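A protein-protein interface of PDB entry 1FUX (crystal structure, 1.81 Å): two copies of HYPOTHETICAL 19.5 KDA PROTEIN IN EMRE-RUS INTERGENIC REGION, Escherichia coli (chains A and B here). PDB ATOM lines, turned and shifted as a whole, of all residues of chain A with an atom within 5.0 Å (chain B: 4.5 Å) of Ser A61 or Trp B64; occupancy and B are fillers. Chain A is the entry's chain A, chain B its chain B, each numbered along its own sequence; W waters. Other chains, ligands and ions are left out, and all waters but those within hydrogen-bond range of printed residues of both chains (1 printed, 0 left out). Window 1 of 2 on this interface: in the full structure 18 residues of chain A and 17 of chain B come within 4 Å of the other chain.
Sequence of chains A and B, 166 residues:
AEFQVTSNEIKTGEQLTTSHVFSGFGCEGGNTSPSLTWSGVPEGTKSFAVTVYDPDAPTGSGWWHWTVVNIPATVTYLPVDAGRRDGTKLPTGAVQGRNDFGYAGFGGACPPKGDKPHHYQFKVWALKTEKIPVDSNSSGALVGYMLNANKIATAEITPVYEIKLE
Among the printed residues, pairs that only touch across the chains: Tyr A53 with Ser B61 (3.9 Å), Thr A59 with Trp B64 (3.9 Å), Thr A59 with Ala B141 (3.2 Å), Ser A61 with Tyr B53 (3.8 Å), Ser A61 with Ser B61 (3.5 Å), Ser A61 with Ala B141 (3.6 Å), Gly A62 with Ala B141 (3.7 Å) and Trp A63 with Ala B141 (3.7 Å).
OH of Tyr A53 lies within hydrogen-bond range of O of Ser A61 (2.7 Å). OG1 of Thr A59 lies within hydrogen-bond range of N of Ser A61 (3.0 Å). The backbone carbonyl oxygen (O) of Gly A62 lies within hydrogen-bond range of the side-chain hydroxyl (OG1) of Thr A59, at 2.8 Å. The backbone carbonyl oxygen (O) of Ser B61 lies within hydrogen-bond range of the side-chain hydroxyl (OH) of Tyr B53 (2.6 Å). The backbone NH (N) of Trp B64 is in hydrogen-bond range of the side-chain carboxylate (OD2) of Asp B100 (2.8 Å).
Ser A61 touches four residues of chain B. Trp B64 touches just these residues of chain A: Thr A59 and Ser A61. Printed residues of chain B within 4 Å of Trp A63: Ala B141 (3.7 Å). Of the printed residues of chain B, Gly A60 touches Tyr B53 (3.4 Å). The nearest printed residue of chain B that does not touch Ser A61 is Gly B140 (4.7 Å). The nearest residue of chain A that does not touch Trp B64 is Gly A60 (4.6 Å).
Tyr A53 touches Ser B61, and with the chains exchanged Ser A61 touches Tyr B53. Ser A61 touches its own counterpart, Ser B61. Positions printed for both chains: 53, 61 and 63.
Hydrophobic or aromatic side chains of chain B that line the printed part of chain A: Tyr B53, Trp B64 and Ala B141. Of the 6 printed residues of chain A, 6 touch a printed residue of chain B. Hydrophobic or aromatic side chains of chain A within 4 Å of the printed part of chain B: Tyr A53 and Trp A63.
The side-chain hydroxyl (OH) of Tyr B53 sits at hydrogen-bond distance from the backbone carbonyl oxygen (O) of Gly A60, at 3.4 Å. The side-chain hydroxyl (OG) of Ser A61 lies within hydrogen-bond range of the indole nitrogen (NE1) of Trp B64, at 2.9 Å.
Water W1 lies within hydrogen-bond range of the side-chain hydroxyl of Tyr B53 (2.9 Å) and the backbone carbonyl oxygen of Gly A60 (3.2 Å).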
ATOM      1  N   TYR A  53     -23.292  19.369  19.257  1.00  0.00           N
ATOM      2  CA  TYR A  53     -23.365  20.051  17.959  1.00  0.00           C
ATOM      3  C   TYR A  53     -22.176  20.952  17.710  1.00  0.00           C
ATOM      4  O   TYR A  53     -21.711  21.588  18.661  1.00  0.00           O
ATOM      5  CB  TYR A  53     -24.630  20.916  17.940  1.00  0.00           C
ATOM      6  CG  TYR A  53     -24.900  21.603  16.586  1.00  0.00           C
ATOM      7  CD1 TYR A  53     -25.458  20.896  15.528  1.00  0.00           C
ATOM      8  CD2 TYR A  53     -24.664  22.931  16.462  1.00  0.00           C
ATOM      9  CE1 TYR A  53     -25.690  21.569  14.315  1.00  0.00           C
ATOM     10  CE2 TYR A  53     -24.940  23.645  15.282  1.00  0.00           C
ATOM     11  CZ  TYR A  53     -25.427  22.915  14.223  1.00  0.00           C
ATOM     12  OH  TYR A  53     -25.726  23.610  13.033  1.00  0.00           O
ATOM     13  N   THR A  59     -20.205  22.814   6.475  1.00  0.00           N
ATOM     14  CA  THR A  59     -21.166  21.976   5.724  1.00  0.00           C
ATOM     15  C   THR A  59     -22.402  22.745   5.320  1.00  0.00           C
ATOM     16  O   THR A  59     -23.053  22.294   4.361  1.00  0.00           O
ATOM     17  CB  THR A  59     -21.668  20.810   6.610  1.00  0.00           C
ATOM     18  OG1 THR A  59     -22.359  21.546   7.667  1.00  0.00           O
ATOM     19  CG2 THR A  59     -20.633  19.886   7.203  1.00  0.00           C
ATOM     20  N   GLY A  60     -22.609  23.913   5.921  1.00  0.00           N
ATOM     21  CA  GLY A  60     -23.862  24.629   5.683  1.00  0.00           C
ATOM     22  C   GLY A  60     -24.905  24.382   6.766  1.00  0.00           C
ATOM     23  O   GLY A  60     -25.897  25.134   6.830  1.00  0.00           O
ATOM     24  N   SER A  61     -24.726  23.370   7.610  1.00  0.00           N
ATOM     25  CA  SER A  61     -25.703  23.064   8.661  1.00  0.00           C
ATOM     26  C   SER A  61     -25.002  22.569   9.939  1.00  0.00           C
ATOM     27  O   SER A  61     -25.721  22.032  10.792  1.00  0.00           O
ATOM     28  CB  SER A  61     -26.652  21.921   8.258  1.00  0.00           C
ATOM     29  OG  SER A  61     -25.970  20.718   7.881  1.00  0.00           O
ATOM     30  N   GLY A  62     -23.732  22.874  10.085  1.00  0.00           N
ATOM     31  CA  GLY A  62     -22.946  22.439  11.252  1.00  0.00           C
ATOM     32  C   GLY A  62     -22.853  20.904  11.225  1.00  0.00           C
ATOM     33  O   GLY A  62     -22.904  20.318  10.139  1.00  0.00           O
ATOM     34  N   TRP A  63     -22.780  20.280  12.389  1.00  0.00           N
ATOM     35  CA  TRP A  63     -22.621  18.824  12.471  1.00  0.00           C
ATOM     36  C   TRP A  63     -23.228  18.339  13.778  1.00  0.00           C
ATOM     37  O   TRP A  63     -22.889  18.808  14.855  1.00  0.00           O
ATOM     38  CB  TRP A  63     -21.137  18.464  12.401  1.00  0.00           C
ATOM     39  CG  TRP A  63     -20.941  16.987  12.093  1.00  0.00           C
ATOM     40  CD1 TRP A  63     -20.884  15.963  12.989  1.00  0.00           C
ATOM     41  CD2 TRP A  63     -20.798  16.419  10.788  1.00  0.00           C
ATOM     42  NE1 TRP A  63     -20.730  14.758  12.320  1.00  0.00           N
ATOM     43  CE2 TRP A  63     -20.626  15.031  10.970  1.00  0.00           C
ATOM     44  CE3 TRP A  63     -20.750  16.956   9.497  1.00  0.00           C
ATOM     45  CZ2 TRP A  63     -20.421  14.147   9.902  1.00  0.00           C
ATOM     46  CZ3 TRP A  63     -20.555  16.073   8.437  1.00  0.00           C
ATOM     47  CH2 TRP A  63     -20.395  14.699   8.636  1.00  0.00           C
ATOM     48  N   THR B  51     -28.822  20.900  -4.021  1.00  0.00           N
ATOM     49  CA  THR B  51     -29.245  20.753  -2.621  1.00  0.00           C
ATOM     50  C   THR B  51     -30.406  21.698  -2.420  1.00  0.00           C
ATOM     51  O   THR B  51     -30.526  22.738  -3.106  1.00  0.00           O
ATOM     52  CB  THR B  51     -28.119  21.163  -1.645  1.00  0.00           C
ATOM     53  OG1 THR B  51     -27.604  22.453  -1.928  1.00  0.00           O
ATOM     54  CG2 THR B  51     -26.986  20.139  -1.717  1.00  0.00           C
ATOM     55  N   VAL B  52     -31.296  21.396  -1.483  1.00  0.00           N
ATOM     56  CA  VAL B  52     -32.424  22.295  -1.124  1.00  0.00           C
ATOM     57  C   VAL B  52     -32.330  22.336   0.407  1.00  0.00           C
ATOM     58  O   VAL B  52     -32.370  21.275   1.008  1.00  0.00           O
ATOM     59  CB  VAL B  52     -33.791  21.744  -1.563  1.00  0.00           C
ATOM     60  CG1 VAL B  52     -34.928  22.643  -1.077  1.00  0.00           C
ATOM     61  CG2 VAL B  52     -33.802  21.543  -3.076  1.00  0.00           C
ATOM     62  N   TYR B  53     -32.349  23.545   0.966  1.00  0.00           N
ATOM     63  CA  TYR B  53     -32.140  23.730   2.406  1.00  0.00           C
ATOM     64  C   TYR B  53     -32.958  24.912   2.924  1.00  0.00           C
ATOM     65  O   TYR B  53     -33.043  25.925   2.203  1.00  0.00           O
ATOM     66  CB  TYR B  53     -30.641  23.967   2.605  1.00  0.00           C
ATOM     67  CG  TYR B  53     -30.219  24.244   4.040  1.00  0.00           C
ATOM     68  CD1 TYR B  53     -30.138  23.150   4.934  1.00  0.00           C
ATOM     69  CD2 TYR B  53     -29.965  25.508   4.497  1.00  0.00           C
ATOM     70  CE1 TYR B  53     -29.728  23.391   6.240  1.00  0.00           C
ATOM     71  CE2 TYR B  53     -29.566  25.752   5.818  1.00  0.00           C
ATOM     72  CZ  TYR B  53     -29.420  24.657   6.660  1.00  0.00           C
ATOM     73  OH  TYR B  53     -29.066  24.873   8.000  1.00  0.00           O
ATOM     74  N   SER B  61     -30.386  23.489  13.189  1.00  0.00           N
ATOM     75  CA  SER B  61     -29.503  23.205  12.029  1.00  0.00           C
ATOM     76  C   SER B  61     -30.239  23.458  10.711  1.00  0.00           C
ATOM     77  O   SER B  61     -29.730  22.995   9.675  1.00  0.00           O
ATOM     78  CB  SER B  61     -28.983  21.771  12.076  1.00  0.00           C
ATOM     79  OG  SER B  61     -30.031  20.800  12.109  1.00  0.00           O
ATOM     80  N   TRP B  63     -33.042  22.703   7.880  1.00  0.00           N
ATOM     81  CA  TRP B  63     -33.621  21.475   7.376  1.00  0.00           C
ATOM     82  C   TRP B  63     -33.143  21.159   5.956  1.00  0.00           C
ATOM     83  O   TRP B  63     -33.256  21.991   5.065  1.00  0.00           O
ATOM     84  CB  TRP B  63     -35.143  21.554   7.318  1.00  0.00           C
ATOM     85  CG  TRP B  63     -35.838  20.248   7.234  1.00  0.00           C
ATOM     86  CD1 TRP B  63     -36.273  19.554   6.131  1.00  0.00           C
ATOM     87  CD2 TRP B  63     -36.201  19.466   8.378  1.00  0.00           C
ATOM     88  NE1 TRP B  63     -36.872  18.387   6.530  1.00  0.00           N
ATOM     89  CE2 TRP B  63     -36.864  18.323   7.907  1.00  0.00           C
ATOM     90  CE3 TRP B  63     -36.019  19.652   9.762  1.00  0.00           C
ATOM     91  CZ2 TRP B  63     -37.358  17.336   8.763  1.00  0.00           C
ATOM     92  CZ3 TRP B  63     -36.556  18.685  10.602  1.00  0.00           C
ATOM     93  CH2 TRP B  63     -37.159  17.517  10.101  1.00  0.00           C
ATOM     94  N   TRP B  64     -32.618  19.970   5.752  1.00  0.00           N
ATOM     95  CA  TRP B  64     -32.201  19.553   4.402  1.00  0.00           C
ATOM     96  C   TRP B  64     -33.368  18.818   3.713  1.00  0.00           C
ATOM     97  O   TRP B  64     -33.856  17.773   4.157  1.00  0.00           O
ATOM     98  CB  TRP B  64     -31.105  18.470   4.524  1.00  0.00           C
ATOM     99  CG  TRP B  64     -29.789  19.042   4.963  1.00  0.00           C
ATOM    100  CD1 TRP B  64     -29.193  18.921   6.184  1.00  0.00           C
ATOM    101  CD2 TRP B  64     -28.921  19.847   4.157  1.00  0.00           C
ATOM    102  NE1 TRP B  64     -28.007  19.630   6.200  1.00  0.00           N
ATOM    103  CE2 TRP B  64     -27.808  20.179   4.948  1.00  0.00           C
ATOM    104  CE3 TRP B  64     -28.969  20.294   2.828  1.00  0.00           C
ATOM    105  CZ2 TRP B  64     -26.731  20.894   4.458  1.00  0.00           C
ATOM    106  CZ3 TRP B  64     -27.918  21.034   2.338  1.00  0.00           C
ATOM    107  CH2 TRP B  64     -26.802  21.363   3.158  1.00  0.00           C
ATOM    108  N   HIS B  65     -33.889  19.391   2.622  1.00  0.00           N
ATOM    109  CA  HIS B  65     -35.041  18.820   1.937  1.00  0.00           C
ATOM    110  C   HIS B  65     -34.635  17.905   0.800  1.00  0.00           C
ATOM    111  O   HIS B  65     -35.425  17.044   0.361  1.00  0.00           O
ATOM    112  CB  HIS B  65     -35.781  20.080   1.298  1.00  0.00           C
ATOM    113  CG  HIS B  65     -36.567  20.790   2.353  1.00  0.00           C
ATOM    114  ND1 HIS B  65     -37.877  20.482   2.638  1.00  0.00           N
ATOM    115  CD2 HIS B  65     -36.204  21.768   3.227  1.00  0.00           C
ATOM    116  CE1 HIS B  65     -38.331  21.234   3.638  1.00  0.00           C
ATOM    117  NE2 HIS B  65     -37.332  22.033   4.020  1.00  0.00           N
ATOM    118  N   TRP B  66     -33.451  18.130   0.231  1.00  0.00           N
ATOM    119  CA  TRP B  66     -33.076  17.291  -0.945  1.00  0.00           C
ATOM    120  C   TRP B  66     -31.599  17.382  -1.210  1.00  0.00           C
ATOM    121  O   TRP B  66     -30.994  18.485  -1.179  1.00  0.00           O
ATOM    122  CB  TRP B  66     -33.786  17.894  -2.200  1.00  0.00           C
ATOM    123  CG  TRP B  66     -33.691  17.032  -3.437  1.00  0.00           C
ATOM    124  CD1 TRP B  66     -33.479  15.670  -3.488  1.00  0.00           C
ATOM    125  CD2 TRP B  66     -33.951  17.423  -4.781  1.00  0.00           C
ATOM    126  NE1 TRP B  66     -33.520  15.214  -4.782  1.00  0.00           N
ATOM    127  CE2 TRP B  66     -33.775  16.297  -5.609  1.00  0.00           C
ATOM    128  CE3 TRP B  66     -34.174  18.669  -5.405  1.00  0.00           C
ATOM    129  CZ2 TRP B  66     -33.927  16.311  -6.994  1.00  0.00           C
ATOM    130  CZ3 TRP B  66     -34.322  18.703  -6.777  1.00  0.00           C
ATOM    131  CH2 TRP B  66     -34.184  17.548  -7.551  1.00  0.00           C
ATOM    132  N   THR B  67     -30.946  16.237  -1.504  1.00  0.00           N
ATOM    133  CA  THR B  67     -29.574  16.296  -1.947  1.00  0.00           C
ATOM    134  C   THR B  67     -29.443  15.275  -3.112  1.00  0.00           C
ATOM    135  O   THR B  67     -29.951  14.165  -3.077  1.00  0.00           O
ATOM    136  CB  THR B  67     -28.469  15.988  -0.951  1.00  0.00           C
ATOM    137  OG1 THR B  67     -28.571  14.613  -0.505  1.00  0.00           O
ATOM    138  CG2 THR B  67     -28.509  16.931   0.241  1.00  0.00           C
ATOM    139  N   ASN B  99     -32.417  13.016   3.251  1.00  0.00           N
ATOM    140  CA  ASN B  99     -32.936  14.316   3.691  1.00  0.00           C
ATOM    141  C   ASN B  99     -33.263  14.263   5.169  1.00  0.00           C
ATOM    142  O   ASN B  99     -33.185  13.195   5.845  1.00  0.00           O
ATOM    143  CB  ASN B  99     -34.125  14.775   2.825  1.00  0.00           C
ATOM    144  CG  ASN B  99     -35.351  13.889   2.943  1.00  0.00           C
ATOM    145  OD1 ASN B  99     -35.648  13.455   4.040  1.00  0.00           O
ATOM    146  ND2 ASN B  99     -36.112  13.667   1.859  1.00  0.00           N
ATOM    147  N   ASP B 100     -33.641  15.407   5.752  1.00  0.00           N
ATOM    148  CA  ASP B 100     -33.979  15.434   7.169  1.00  0.00           C
ATOM    149  C   ASP B 100     -35.289  14.765   7.528  1.00  0.00           C
ATOM    150  O   ASP B 100     -35.560  14.470   8.702  1.00  0.00           O
ATOM    151  CB  ASP B 100     -33.889  16.813   7.797  1.00  0.00           C
ATOM    152  CG  ASP B 100     -32.456  17.181   8.072  1.00  0.00           C
ATOM    153  OD1 ASP B 100     -31.527  16.338   8.267  1.00  0.00           O
ATOM    154  OD2 ASP B 100     -32.160  18.397   8.028  1.00  0.00           O
ATOM    155  N   GLY B 140     -27.426  15.134   5.248  1.00  0.00           N
ATOM    156  CA  GLY B 140     -27.284  16.438   4.520  1.00  0.00           C
ATOM    157  C   GLY B 140     -25.955  17.091   4.843  1.00  0.00           C
ATOM    158  O   GLY B 140     -25.294  17.680   3.991  1.00  0.00           O
ATOM    159  N   ALA B 141     -25.567  17.072   6.140  1.00  0.00           N
ATOM    160  CA  ALA B 141     -24.283  17.677   6.499  1.00  0.00           C
ATOM    161  C   ALA B 141     -23.088  16.992   5.862  1.00  0.00           C
ATOM    162  O   ALA B 141     -22.155  17.726   5.480  1.00  0.00           O
ATOM    163  CB  ALA B 141     -24.142  17.580   8.059  1.00  0.00           C
HETATM  164  O   HOH W   1     -27.479  27.177   8.703  1.00  0.00           O
